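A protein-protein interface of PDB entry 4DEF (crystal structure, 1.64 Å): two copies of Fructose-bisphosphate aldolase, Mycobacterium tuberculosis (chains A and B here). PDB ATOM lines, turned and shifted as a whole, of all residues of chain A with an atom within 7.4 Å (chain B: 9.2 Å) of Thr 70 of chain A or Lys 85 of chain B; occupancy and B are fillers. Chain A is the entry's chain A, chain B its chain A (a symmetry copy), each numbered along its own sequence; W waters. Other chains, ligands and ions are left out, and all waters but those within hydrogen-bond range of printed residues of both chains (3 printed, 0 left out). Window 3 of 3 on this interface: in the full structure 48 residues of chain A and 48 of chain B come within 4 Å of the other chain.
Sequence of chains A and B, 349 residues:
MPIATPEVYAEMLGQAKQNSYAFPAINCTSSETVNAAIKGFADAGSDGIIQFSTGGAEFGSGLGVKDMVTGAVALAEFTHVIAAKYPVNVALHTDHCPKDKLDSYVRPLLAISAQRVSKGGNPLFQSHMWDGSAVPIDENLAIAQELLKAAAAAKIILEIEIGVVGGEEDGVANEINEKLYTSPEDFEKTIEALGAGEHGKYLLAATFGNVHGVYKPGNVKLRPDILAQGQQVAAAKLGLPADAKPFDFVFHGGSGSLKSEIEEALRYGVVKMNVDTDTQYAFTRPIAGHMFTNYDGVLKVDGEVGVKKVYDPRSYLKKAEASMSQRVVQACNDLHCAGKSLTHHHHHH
The side-chain amide nitrogen of Asn 35 of chain B lies within hydrogen-bond range of the backbone carbonyl oxygen of Gly 60 of chain A (2.9 Å).
N of Gly 62 of chain A sits close to ND2 of Asn 35 of chain B (3.3 Å).
The side-chain hydroxyl (OH) of Tyr 86 of chain B lies close to the backbone NH (N) of Gly 64 of chain A.
OG of Ser 61 of chain A lies within hydrogen-bond range of N of Lys 66 of chain A (3.1 Å).
The backbone NH of Asp 67 of chain A sits at hydrogen-bond distance from the side-chain hydroxyl of Ser 61 of chain A (2.9 Å).
The side-chain carboxylate (OD2) of Asp 67 of chain A lies within hydrogen-bond range of the side-chain hydroxyl (OG1) of Thr 70 of chain A (2.9 Å).
O of Glu 58 of chain A sits at hydrogen-bond distance from OG of Ser 61 of chain A.
Gly 60 of chain A touches Phe 78 of chain B (O to CZ, 3.5 Å).
CD1 of Ile 82 of chain B touches O of Gly 60 of chain A (3.96 Å).
O of Ser 61 of chain A touches OD1 of Asn 35 of chain B, 3.7 Å away.
O of Ser 61 of chain A touches CD1 of Ile 82 of chain B, at 3.9 Å.
CG2 of Val 65 of chain A touches CE2 of Tyr 86 of chain B (3.4 Å).
Thr 70 of chain A touches Val 81 of chain B (O to CG1, 3.6 Å).
Thr 70 of chain A touches Lys 85 of chain B.
Val 73 of chain A touches Val 81 of chain B.
CG1 of Val 81 of chain B touches CB of Ala 74 of chain A, 3.8 Å away.
Ile 82 of chain B touches Ala 74 of chain A.
Of the printed residues of chain B, Gly 60 of chain A touches Asn 35 (2.9 Å), Phe 78 (3.5 Å) and Ile 82 (3.96 Å).
Of the printed residues of chain B, Gly 62 of chain A touches Asn 35.
No residue of chain B comes within 4 Å of Val 69 of chain A.
Thr 70 of chain A touches two residues of chain B.
Of the printed residues of chain B, Val 73 of chain A touches Val 81.
Ile 3 of chain B touches none of the printed residues of chain A.
Of the printed residues of chain A, Lys 85 of chain B touches Val 65 (3.9 Å) and Thr 70 (3.5 Å).
The nearest printed residue of chain A that does not touch Ile 82 of chain B is Thr 70 of chain A (4.1 Å).
Hydrophobic or aromatic side chains of chain B that line the printed part of chain A: Phe 78, Val 81, Ile 82 and Tyr 86.
Of the 22 printed residues of chain A, 8 touch a printed residue of chain B.
Printed residues of chain A that touch a printed residue of chain B: Gly 60, Ser 61, Gly 62, Gly 64, Val 65, Thr 70, Val 73 and Ala 74.
No position is printed for both chains.
Of the 15 pairs that touch across the chains among the printed residues, none has its exchanged pair printed and touching as well.
Water W2 lies within hydrogen-bond range of OH of Tyr 86 of chain B, O of Ser 61 of chain A and OD1 of Asn 35 of chain B.
Water W1 lies within hydrogen-bond range of O of Lys 85 of chain B (2.9 Å) and O of Gly 64 of chain A (3.0 Å).
Water W3 lies within hydrogen-bond range of the backbone NH of Gly 64 of chain A (2.9 Å), the side-chain hydroxyl of Tyr 86 of chain B (2.9 Å) and the backbone carbonyl oxygen of Asn 35 of chain B (3.3 Å).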
ATOM      1  N   ALA A  57      -3.968  -9.669 -13.715  1.00  0.00           N
ATOM      2  CA  ALA A  57      -2.556  -9.498 -14.041  1.00  0.00           C
ATOM      3  C   ALA A  57      -1.668 -10.399 -13.184  1.00  0.00           C
ATOM      4  O   ALA A  57      -0.765 -11.069 -13.693  1.00  0.00           O
ATOM      5  CB  ALA A  57      -2.150  -8.033 -13.872  1.00  0.00           C
ATOM      6  N   GLU A  58      -1.945 -10.442 -11.884  1.00  0.00           N
ATOM      7  CA  GLU A  58      -1.201 -11.321 -11.003  1.00  0.00           C
ATOM      8  C   GLU A  58      -1.332 -12.789 -11.446  1.00  0.00           C
ATOM      9  O   GLU A  58      -0.337 -13.510 -11.507  1.00  0.00           O
ATOM     10  CB  GLU A  58      -1.659 -11.145  -9.552  1.00  0.00           C
ATOM     11  CG  GLU A  58      -0.791 -11.914  -8.573  1.00  0.00           C
ATOM     12  CD  GLU A  58      -1.308 -11.862  -7.153  1.00  0.00           C
ATOM     13  OE1 GLU A  58      -1.303 -10.759  -6.574  1.00  0.00           O
ATOM     14  OE2 GLU A  58      -1.701 -12.926  -6.615  1.00  0.00           O
ATOM     15  N   GLY A  60      -2.139 -13.831 -14.496  1.00  0.00           N
ATOM     16  CA  GLY A  60      -1.410 -13.908 -15.767  1.00  0.00           C
ATOM     17  C   GLY A  60       0.091 -14.108 -15.651  1.00  0.00           C
ATOM     18  O   GLY A  60       0.718 -14.717 -16.527  1.00  0.00           O
ATOM     19  N   SER A  61       0.684 -13.600 -14.565  1.00  0.00           N
ATOM     20  CA  SER A  61       2.116 -13.722 -14.360  1.00  0.00           C
ATOM     21  C   SER A  61       2.539 -15.103 -13.853  1.00  0.00           C
ATOM     22  O   SER A  61       3.728 -15.412 -13.848  1.00  0.00           O
ATOM     23  CB  SER A  61       2.612 -12.627 -13.408  1.00  0.00           C
ATOM     24  OG  SER A  61       2.214 -12.893 -12.071  1.00  0.00           O
ATOM     25  N   GLY A  62       1.565 -15.918 -13.429  1.00  0.00           N
ATOM     26  CA  GLY A  62       1.825 -17.256 -12.895  1.00  0.00           C
ATOM     27  C   GLY A  62       2.089 -17.283 -11.395  1.00  0.00           C
ATOM     28  O   GLY A  62       2.509 -16.280 -10.805  1.00  0.00           O
ATOM     29  N   GLY A  64       4.407 -18.620  -9.747  1.00  0.00           N
ATOM     30  CA  GLY A  64       5.808 -18.449  -9.395  1.00  0.00           C
ATOM     31  C   GLY A  64       6.314 -17.018  -9.403  1.00  0.00           C
ATOM     32  O   GLY A  64       7.439 -16.763  -8.967  1.00  0.00           O
ATOM     33  N   VAL A  65       5.494 -16.089  -9.898  1.00  0.00           N
ATOM     34  CA  VAL A  65       5.902 -14.686 -10.061  1.00  0.00           C
ATOM     35  C   VAL A  65       4.987 -13.759  -9.261  1.00  0.00           C
ATOM     36  O   VAL A  65       5.459 -12.954  -8.444  1.00  0.00           O
ATOM     37  CB  VAL A  65       5.933 -14.276 -11.558  1.00  0.00           C
ATOM     38  CG1 VAL A  65       6.351 -12.822 -11.729  1.00  0.00           C
ATOM     39  CG2 VAL A  65       6.883 -15.167 -12.343  1.00  0.00           C
ATOM     40  N   LYS A  66       3.682 -13.879  -9.501  1.00  0.00           N
ATOM     41  CA  LYS A  66       2.655 -13.071  -8.838  1.00  0.00           C
ATOM     42  C   LYS A  66       3.024 -11.594  -8.883  1.00  0.00           C
ATOM     43  O   LYS A  66       3.090 -10.931  -7.844  1.00  0.00           O
ATOM     44  CB  LYS A  66       2.408 -13.544  -7.396  1.00  0.00           C
ATOM     45  CG  LYS A  66       1.878 -14.966  -7.286  1.00  0.00           C
ATOM     46  CD  LYS A  66       1.586 -15.337  -5.839  1.00  0.00           C
ATOM     47  CE  LYS A  66       1.051 -16.756  -5.746  1.00  0.00           C
ATOM     48  NZ  LYS A  66       0.833 -17.177  -4.332  1.00  0.00           N
ATOM     49  N   ASP A  67       3.299 -11.096 -10.089  1.00  0.00           N
ATOM     50  CA  ASP A  67       3.681  -9.695 -10.273  1.00  0.00           C
ATOM     51  C   ASP A  67       2.772  -9.067 -11.308  1.00  0.00           C
ATOM     52  O   ASP A  67       2.723  -9.526 -12.457  1.00  0.00           O
ATOM     53  CB  ASP A  67       5.138  -9.568 -10.718  1.00  0.00           C
ATOM     54  CG  ASP A  67       5.584  -8.121 -10.821  1.00  0.00           C
ATOM     55  OD1 ASP A  67       5.834  -7.502  -9.764  1.00  0.00           O
ATOM     56  OD2 ASP A  67       5.662  -7.600 -11.948  1.00  0.00           O
ATOM     57  N   MET A  68       2.064  -8.018 -10.901  1.00  0.00           N
ATOM     58  CA  MET A  68       1.049  -7.388 -11.745  1.00  0.00           C
ATOM     59  C   MET A  68       1.625  -6.824 -13.039  1.00  0.00           C
ATOM     60  O   MET A  68       1.033  -6.998 -14.099  1.00  0.00           O
ATOM     61  CB  MET A  68       0.322  -6.277 -10.992  1.00  0.00           C
ATOM     62  CG  MET A  68      -0.565  -6.753  -9.854  1.00  0.00           C
ATOM     63  SD  MET A  68      -1.189  -5.348  -8.902  1.00  0.00           S
ATOM     64  CE  MET A  68       0.301  -4.734  -8.134  1.00  0.00           C
ATOM     65  N   VAL A  69       2.760  -6.128 -12.963  1.00  0.00           N
ATOM     66  CA  VAL A  69       3.348  -5.557 -14.174  1.00  0.00           C
ATOM     67  C   VAL A  69       3.724  -6.659 -15.148  1.00  0.00           C
ATOM     68  O   VAL A  69       3.408  -6.568 -16.335  1.00  0.00           O
ATOM     69  CB  VAL A  69       4.538  -4.623 -13.875  1.00  0.00           C
ATOM     70  CG1 VAL A  69       5.302  -4.270 -15.144  1.00  0.00           C
ATOM     71  CG2 VAL A  69       3.997  -3.354 -13.236  1.00  0.00           C
ATOM     72  N   THR A  70       4.377  -7.700 -14.634  1.00  0.00           N
ATOM     73  CA  THR A  70       4.813  -8.816 -15.476  1.00  0.00           C
ATOM     74  C   THR A  70       3.633  -9.455 -16.218  1.00  0.00           C
ATOM     75  O   THR A  70       3.715  -9.674 -17.434  1.00  0.00           O
ATOM     76  CB  THR A  70       5.564  -9.886 -14.671  1.00  0.00           C
ATOM     77  OG1 THR A  70       6.706  -9.284 -14.064  1.00  0.00           O
ATOM     78  CG2 THR A  70       6.041 -11.011 -15.592  1.00  0.00           C
ATOM     79  N   GLY A  71       2.564  -9.747 -15.483  1.00  0.00           N
ATOM     80  CA  GLY A  71       1.359 -10.373 -16.055  1.00  0.00           C
ATOM     81  C   GLY A  71       0.697  -9.486 -17.091  1.00  0.00           C
ATOM     82  O   GLY A  71       0.326  -9.949 -18.184  1.00  0.00           O
ATOM     83  N   ALA A  72       0.569  -8.195 -16.781  1.00  0.00           N
ATOM     84  CA  ALA A  72      -0.054  -7.263 -17.727  1.00  0.00           C
ATOM     85  C   ALA A  72       0.773  -7.132 -19.001  1.00  0.00           C
ATOM     86  O   ALA A  72       0.222  -7.140 -20.117  1.00  0.00           O
ATOM     87  CB  ALA A  72      -0.265  -5.892 -17.094  1.00  0.00           C
ATOM     88  N   VAL A  73       2.091  -7.023 -18.853  1.00  0.00           N
ATOM     89  CA  VAL A  73       2.957  -6.889 -20.016  1.00  0.00           C
ATOM     90  C   VAL A  73       2.919  -8.166 -20.838  1.00  0.00           C
ATOM     91  O   VAL A  73       2.815  -8.091 -22.066  1.00  0.00           O
ATOM     92  CB  VAL A  73       4.409  -6.534 -19.647  1.00  0.00           C
ATOM     93  CG1 VAL A  73       5.321  -6.613 -20.865  1.00  0.00           C
ATOM     94  CG2 VAL A  73       4.465  -5.133 -19.044  1.00  0.00           C
ATOM     95  N   ALA A  74       2.989  -9.316 -20.161  1.00  0.00           N
ATOM     96  CA  ALA A  74       3.015 -10.603 -20.865  1.00  0.00           C
ATOM     97  C   ALA A  74       1.723 -10.783 -21.670  1.00  0.00           C
ATOM     98  O   ALA A  74       1.774 -11.136 -22.869  1.00  0.00           O
ATOM     99  CB  ALA A  74       3.210 -11.751 -19.880  1.00  0.00           C
ATOM    100  N   LEU A  75       0.589 -10.505 -21.035  1.00  0.00           N
ATOM    101  CA  LEU A  75      -0.711 -10.656 -21.712  1.00  0.00           C
ATOM    102  C   LEU A  75      -0.898  -9.596 -22.794  1.00  0.00           C
ATOM    103  O   LEU A  75      -1.458  -9.886 -23.861  1.00  0.00           O
ATOM    104  CB  LEU A  75      -1.874 -10.643 -20.709  1.00  0.00           C
ATOM    105  CG  LEU A  75      -1.998 -11.866 -19.793  1.00  0.00           C
ATOM    106  CD1 LEU A  75      -3.025 -11.584 -18.712  1.00  0.00           C
ATOM    107  CD2 LEU A  75      -2.359 -13.131 -20.567  1.00  0.00           C
ATOM    108  N   ALA A  76      -0.413  -8.379 -22.546  1.00  0.00           N
ATOM    109  CA  ALA A  76      -0.470  -7.327 -23.575  1.00  0.00           C
ATOM    110  C   ALA A  76       0.356  -7.686 -24.799  1.00  0.00           C
ATOM    111  O   ALA A  76      -0.102  -7.459 -25.937  1.00  0.00           O
ATOM    112  CB  ALA A  76      -0.031  -5.978 -23.029  1.00  0.00           C
ATOM    113  N   SER A 104       3.038  -0.018  -8.191  1.00  0.00           N
ATOM    114  CA  SER A 104       3.363  -1.382  -8.638  1.00  0.00           C
ATOM    115  C   SER A 104       2.500  -1.875  -9.807  1.00  0.00           C
ATOM    116  O   SER A 104       2.573  -3.049 -10.195  1.00  0.00           O
ATOM    117  CB  SER A 104       3.330  -2.371  -7.463  1.00  0.00           C
ATOM    118  OG  SER A 104       2.077  -2.367  -6.813  1.00  0.00           O
ATOM    119  N   TYR A 105       1.698  -0.985 -10.378  1.00  0.00           N
ATOM    120  CA  TYR A 105       0.871  -1.355 -11.533  1.00  0.00           C
ATOM    121  C   TYR A 105       0.825  -0.221 -12.556  1.00  0.00           C
ATOM    122  O   TYR A 105       1.613  -0.211 -13.497  1.00  0.00           O
ATOM    123  CB  TYR A 105      -0.522  -1.787 -11.071  1.00  0.00           C
ATOM    124  CG  TYR A 105      -1.334  -2.570 -12.088  1.00  0.00           C
ATOM    125  CD1 TYR A 105      -0.721  -3.505 -12.925  1.00  0.00           C
ATOM    126  CD2 TYR A 105      -2.711  -2.401 -12.186  1.00  0.00           C
ATOM    127  CE1 TYR A 105      -1.461  -4.235 -13.843  1.00  0.00           C
ATOM    128  CE2 TYR A 105      -3.467  -3.138 -13.100  1.00  0.00           C
ATOM    129  CZ  TYR A 105      -2.821  -4.043 -13.929  1.00  0.00           C
ATOM    130  OH  TYR A 105      -3.546  -4.783 -14.835  1.00  0.00           O
ATOM    131  N   LEU A 109       3.648   0.777 -15.647  1.00  0.00           N
ATOM    132  CA  LEU A 109       3.124   0.557 -16.992  1.00  0.00           C
ATOM    133  C   LEU A 109       3.137   1.852 -17.793  1.00  0.00           C
ATOM    134  O   LEU A 109       3.473   1.839 -18.977  1.00  0.00           O
ATOM    135  CB  LEU A 109       1.718  -0.072 -16.980  1.00  0.00           C
ATOM    136  CG  LEU A 109       1.641  -1.550 -16.559  1.00  0.00           C
ATOM    137  CD1 LEU A 109       0.199  -1.993 -16.377  1.00  0.00           C
ATOM    138  CD2 LEU A 109       2.370  -2.479 -17.526  1.00  0.00           C
ATOM    139  N   ILE A 112       6.630   2.350 -19.026  1.00  0.00           N
ATOM    140  CA  ILE A 112       6.947   1.490 -20.171  1.00  0.00           C
ATOM    141  C   ILE A 112       6.435   2.140 -21.453  1.00  0.00           C
ATOM    142  O   ILE A 112       7.158   2.213 -22.455  1.00  0.00           O
ATOM    143  CB  ILE A 112       6.375   0.054 -20.006  1.00  0.00           C
ATOM    144  CG1 ILE A 112       7.204  -0.729 -18.983  1.00  0.00           C
ATOM    145  CG2 ILE A 112       6.366  -0.694 -21.343  1.00  0.00           C
ATOM    146  CD1 ILE A 112       6.541  -2.001 -18.484  1.00  0.00           C
ATOM    147  N   PRO B   2      15.626 -16.804 -17.068  1.00  0.00           N
ATOM    148  CA  PRO B   2      15.550 -16.112 -18.351  1.00  0.00           C
ATOM    149  C   PRO B   2      15.286 -17.087 -19.487  1.00  0.00           C
ATOM    150  O   PRO B   2      15.403 -18.294 -19.307  1.00  0.00           O
ATOM    151  CB  PRO B   2      16.965 -15.512 -18.500  1.00  0.00           C
ATOM    152  CG  PRO B   2      17.832 -16.385 -17.656  1.00  0.00           C
ATOM    153  CD  PRO B   2      16.967 -16.670 -16.465  1.00  0.00           C
ATOM    154  N   ILE B   3      14.924 -16.559 -20.655  1.00  0.00           N
ATOM    155  CA  ILE B   3      14.936 -17.376 -21.864  1.00  0.00           C
ATOM    156  C   ILE B   3      16.386 -17.813 -22.099  1.00  0.00           C
ATOM    157  O   ILE B   3      17.309 -17.015 -21.923  1.00  0.00           O
ATOM    158  CB  ILE B   3      14.425 -16.598 -23.101  1.00  0.00           C
ATOM    159  CG1 ILE B   3      12.924 -16.298 -22.987  1.00  0.00           C
ATOM    160  CG2 ILE B   3      14.710 -17.402 -24.371  1.00  0.00           C
ATOM    161  CD1 ILE B   3      12.032 -17.532 -23.029  1.00  0.00           C
ATOM    162  N   ASN B  35       3.022 -21.016 -17.924  1.00  0.00           N
ATOM    163  CA  ASN B  35       3.304 -20.657 -16.521  1.00  0.00           C
ATOM    164  C   ASN B  35       3.541 -21.867 -15.626  1.00  0.00           C
ATOM    165  O   ASN B  35       4.483 -21.864 -14.811  1.00  0.00           O
ATOM    166  CB  ASN B  35       2.206 -19.769 -15.949  1.00  0.00           C
ATOM    167  CG  ASN B  35       2.379 -18.308 -16.334  1.00  0.00           C
ATOM    168  OD1 ASN B  35       3.485 -17.851 -16.625  1.00  0.00           O
ATOM    169  ND2 ASN B  35       1.293 -17.571 -16.327  1.00  0.00           N
ATOM    170  N   ILE B  38       7.097 -23.445 -16.482  1.00  0.00           N
ATOM    171  CA  ILE B  38       8.272 -22.696 -16.012  1.00  0.00           C
ATOM    172  C   ILE B  38       8.349 -22.784 -14.484  1.00  0.00           C
ATOM    173  O   ILE B  38       9.423 -22.995 -13.924  1.00  0.00           O
ATOM    174  CB  ILE B  38       8.278 -21.225 -16.459  1.00  0.00           C
ATOM    175  CG1 ILE B  38       8.302 -21.148 -17.987  1.00  0.00           C
ATOM    176  CG2 ILE B  38       9.549 -20.555 -15.954  1.00  0.00           C
ATOM    177  CD1 ILE B  38       8.110 -19.746 -18.540  1.00  0.00           C
ATOM    178  N   ALA B  42      11.446 -24.243 -12.259  1.00  0.00           N
ATOM    179  CA  ALA B  42      12.015 -23.420 -11.194  1.00  0.00           C
ATOM    180  C   ALA B  42      11.952 -24.132  -9.842  1.00  0.00           C
ATOM    181  O   ALA B  42      12.927 -24.094  -9.065  1.00  0.00           O
ATOM    182  CB  ALA B  42      11.329 -22.068 -11.125  1.00  0.00           C
ATOM    183  N   GLU B  77       6.195 -14.793 -27.406  1.00  0.00           N
ATOM    184  CA  GLU B  77       6.331 -13.437 -26.857  1.00  0.00           C
ATOM    185  C   GLU B  77       5.891 -13.394 -25.397  1.00  0.00           C
ATOM    186  O   GLU B  77       6.575 -12.790 -24.564  1.00  0.00           O
ATOM    187  CB  GLU B  77       5.593 -12.376 -27.682  1.00  0.00           C
ATOM    188  CG  GLU B  77       6.130 -12.178 -29.104  1.00  0.00           C
ATOM    189  CD  GLU B  77       7.526 -11.592 -29.176  1.00  0.00           C
ATOM    190  OE1 GLU B  77       7.986 -11.319 -30.313  1.00  0.00           O
ATOM    191  OE2 GLU B  77       8.173 -11.397 -28.121  1.00  0.00           O
ATOM    192  N   PHE B  78       4.784 -14.067 -25.090  1.00  0.00           N
ATOM    193  CA  PHE B  78       4.332 -14.204 -23.705  1.00  0.00           C
ATOM    194  C   PHE B  78       5.433 -14.858 -22.860  1.00  0.00           C
ATOM    195  O   PHE B  78       5.745 -14.376 -21.765  1.00  0.00           O
ATOM    196  CB  PHE B  78       3.038 -15.034 -23.644  1.00  0.00           C
ATOM    197  CG  PHE B  78       2.593 -15.365 -22.240  1.00  0.00           C
ATOM    198  CD1 PHE B  78       1.733 -14.512 -21.557  1.00  0.00           C
ATOM    199  CD2 PHE B  78       3.010 -16.542 -21.628  1.00  0.00           C
ATOM    200  CE1 PHE B  78       1.318 -14.817 -20.263  1.00  0.00           C
ATOM    201  CE2 PHE B  78       2.604 -16.848 -20.333  1.00  0.00           C
ATOM    202  CZ  PHE B  78       1.761 -15.980 -19.655  1.00  0.00           C
ATOM    203  N   THR B  79       5.997 -15.959 -23.357  1.00  0.00           N
ATOM    204  CA  THR B  79       6.982 -16.753 -22.592  1.00  0.00           C
ATOM    205  C   THR B  79       8.250 -15.938 -22.330  1.00  0.00           C
ATOM    206  O   THR B  79       8.858 -16.062 -21.258  1.00  0.00           O
ATOM    207  CB  THR B  79       7.335 -18.072 -23.322  1.00  0.00           C
ATOM    208  OG1 THR B  79       6.130 -18.806 -23.578  1.00  0.00           O
ATOM    209  CG2 THR B  79       8.280 -18.943 -22.496  1.00  0.00           C
ATOM    210  N   HIS B  80       8.635 -15.094 -23.297  1.00  0.00           N
ATOM    211  CA  HIS B  80       9.821 -14.228 -23.127  1.00  0.00           C
ATOM    212  C   HIS B  80       9.664 -13.319 -21.938  1.00  0.00           C
ATOM    213  O   HIS B  80      10.597 -13.178 -21.145  1.00  0.00           O
ATOM    214  CB  HIS B  80      10.128 -13.442 -24.398  1.00  0.00           C
ATOM    215  CG  HIS B  80      10.958 -14.215 -25.396  1.00  0.00           C
ATOM    216  ND1 HIS B  80      12.240 -13.904 -25.670  1.00  0.00           N
ATOM    217  CD2 HIS B  80      10.643 -15.317 -26.186  1.00  0.00           C
ATOM    218  CE1 HIS B  80      12.722 -14.766 -26.593  1.00  0.00           C
ATOM    219  NE2 HIS B  80      11.746 -15.630 -26.903  1.00  0.00           N
ATOM    220  N   VAL B  81       8.476 -12.746 -21.767  1.00  0.00           N
ATOM    221  CA  VAL B  81       8.219 -11.847 -20.631  1.00  0.00           C
ATOM    222  C   VAL B  81       8.266 -12.613 -19.301  1.00  0.00           C
ATOM    223  O   VAL B  81       8.913 -12.171 -18.337  1.00  0.00           O
ATOM    224  CB  VAL B  81       6.886 -11.080 -20.801  1.00  0.00           C
ATOM    225  CG1 VAL B  81       6.599 -10.169 -19.604  1.00  0.00           C
ATOM    226  CG2 VAL B  81       6.903 -10.263 -22.091  1.00  0.00           C
ATOM    227  N   ILE B  82       7.582 -13.750 -19.243  1.00  0.00           N
ATOM    228  CA  ILE B  82       7.522 -14.544 -18.008  1.00  0.00           C
ATOM    229  C   ILE B  82       8.893 -15.084 -17.604  1.00  0.00           C
ATOM    230  O   ILE B  82       9.269 -15.007 -16.428  1.00  0.00           O
ATOM    231  CB  ILE B  82       6.562 -15.749 -18.140  1.00  0.00           C
ATOM    232  CG1 ILE B  82       5.139 -15.276 -18.475  1.00  0.00           C
ATOM    233  CG2 ILE B  82       6.567 -16.590 -16.865  1.00  0.00           C
ATOM    234  CD1 ILE B  82       4.526 -14.280 -17.504  1.00  0.00           C
ATOM    235  N   ALA B  83       9.623 -15.658 -18.559  1.00  0.00           N
ATOM    236  CA  ALA B  83      10.852 -16.381 -18.210  1.00  0.00           C
ATOM    237  C   ALA B  83      11.907 -15.449 -17.655  1.00  0.00           C
ATOM    238  O   ALA B  83      12.770 -15.896 -16.903  1.00  0.00           O
ATOM    239  CB  ALA B  83      11.401 -17.149 -19.403  1.00  0.00           C
ATOM    240  N   ALA B  84      11.835 -14.172 -18.024  1.00  0.00           N
ATOM    241  CA  ALA B  84      12.775 -13.159 -17.499  1.00  0.00           C
ATOM    242  C   ALA B  84      12.684 -13.013 -15.975  1.00  0.00           C
ATOM    243  O   ALA B  84      13.619 -12.513 -15.332  1.00  0.00           O
ATOM    244  CB  ALA B  84      12.552 -11.822 -18.187  1.00  0.00           C
ATOM    245  N   LYS B  85      11.574 -13.461 -15.395  1.00  0.00           N
ATOM    246  CA  LYS B  85      11.352 -13.353 -13.950  1.00  0.00           C
ATOM    247  C   LYS B  85      11.748 -14.613 -13.163  1.00  0.00           C
ATOM    248  O   LYS B  85      11.565 -14.669 -11.942  1.00  0.00           O
ATOM    249  CB  LYS B  85       9.889 -12.986 -13.670  1.00  0.00           C
ATOM    250  CG  LYS B  85       9.427 -11.688 -14.319  1.00  0.00           C
ATOM    251  CD  LYS B  85      10.153 -10.468 -13.769  1.00  0.00           C
ATOM    252  CE  LYS B  85       9.670 -10.119 -12.369  1.00  0.00           C
ATOM    253  NZ  LYS B  85      10.283  -8.835 -11.940  1.00  0.00           N
ATOM    254  N   TYR B  86      12.274 -15.628 -13.845  1.00  0.00           N
ATOM    255  CA  TYR B  86      12.693 -16.855 -13.170  1.00  0.00           C
ATOM    256  C   TYR B  86      14.207 -17.078 -13.251  1.00  0.00           C
ATOM    257  O   TYR B  86      14.823 -16.730 -14.253  1.00  0.00           O
ATOM    258  CB  TYR B  86      12.001 -18.056 -13.810  1.00  0.00           C
ATOM    259  CG  TYR B  86      10.552 -18.226 -13.444  1.00  0.00           C
ATOM    260  CD1 TYR B  86      10.183 -18.967 -12.322  1.00  0.00           C
ATOM    261  CD2 TYR B  86       9.541 -17.663 -14.228  1.00  0.00           C
ATOM    262  CE1 TYR B  86       8.855 -19.157 -11.981  1.00  0.00           C
ATOM    263  CE2 TYR B  86       8.207 -17.853 -13.900  1.00  0.00           C
ATOM    264  CZ  TYR B  86       7.874 -18.590 -12.770  1.00  0.00           C
ATOM    265  OH  TYR B  86       6.565 -18.797 -12.428  1.00  0.00           O
ATOM    266  N   PRO B  87      14.806 -17.691 -12.209  1.00  0.00           N
ATOM    267  CA  PRO B  87      16.252 -17.950 -12.181  1.00  0.00           C
ATOM    268  C   PRO B  87      16.652 -19.322 -12.738  1.00  0.00           C
ATOM    269  O   PRO B  87      17.556 -19.997 -12.200  1.00  0.00           O
ATOM    270  CB  PRO B  87      16.562 -17.898 -10.688  1.00  0.00           C
ATOM    271  CG  PRO B  87      15.335 -18.461 -10.053  1.00  0.00           C
ATOM    272  CD  PRO B  87      14.165 -18.079 -10.938  1.00  0.00           C
ATOM    273  N   VAL B  88      15.970 -19.747 -13.791  1.00  0.00           N
ATOM    274  CA  VAL B  88      16.366 -20.927 -14.542  1.00  0.00           C
ATOM    275  C   VAL B  88      16.280 -20.561 -16.006  1.00  0.00           C
ATOM    276  O   VAL B  88      15.663 -19.563 -16.349  1.00  0.00           O
ATOM    277  CB  VAL B  88      15.475 -22.153 -14.248  1.00  0.00           C
ATOM    278  CG1 VAL B  88      15.640 -22.603 -12.798  1.00  0.00           C
ATOM    279  CG2 VAL B  88      14.004 -21.876 -14.560  1.00  0.00           C
ATOM    280  N   VAL B  90      15.054 -21.226 -19.779  1.00  0.00           N
ATOM    281  CA  VAL B  90      13.919 -21.837 -20.459  1.00  0.00           C
ATOM    282  C   VAL B  90      14.138 -21.689 -21.970  1.00  0.00           C
ATOM    283  O   VAL B  90      14.233 -20.570 -22.471  1.00  0.00           O
ATOM    284  CB  VAL B  90      12.619 -21.124 -20.048  1.00  0.00           C
ATOM    285  CG1 VAL B  90      11.415 -21.733 -20.758  1.00  0.00           C
ATOM    286  CG2 VAL B  90      12.433 -21.134 -18.528  1.00  0.00           C
ATOM    287  N   HIS B 345      21.562 -21.383  -8.940  1.00  0.00           N
ATOM    288  CA  HIS B 345      20.834 -20.922  -7.759  1.00  0.00           C
ATOM    289  C   HIS B 345      20.603 -22.080  -6.843  1.00  0.00           C
ATOM    290  O   HIS B 345      19.851 -22.997  -7.167  1.00  0.00           O
ATOM    291  CB  HIS B 345      19.489 -20.334  -8.160  1.00  0.00           C
ATOM    292  CG  HIS B 345      19.546 -18.880  -8.529  1.00  0.00           C
ATOM    293  ND1 HIS B 345      19.145 -17.910  -7.693  1.00  0.00           N
ATOM    294  CD2 HIS B 345      19.977 -18.247  -9.693  1.00  0.00           C
ATOM    295  CE1 HIS B 345      19.307 -16.712  -8.283  1.00  0.00           C
ATOM    296  NE2 HIS B 345      19.813 -16.919  -9.511  1.00  0.00           N
HETATM  297  O   HOH W   1      10.194 -16.121  -9.886  1.00  0.00           O
HETATM  298  O   HOH W   2       4.916 -17.819 -14.290  1.00  0.00           O
HETATM  299  O   HOH W   3       3.828 -19.780 -12.340  1.00  0.00           O
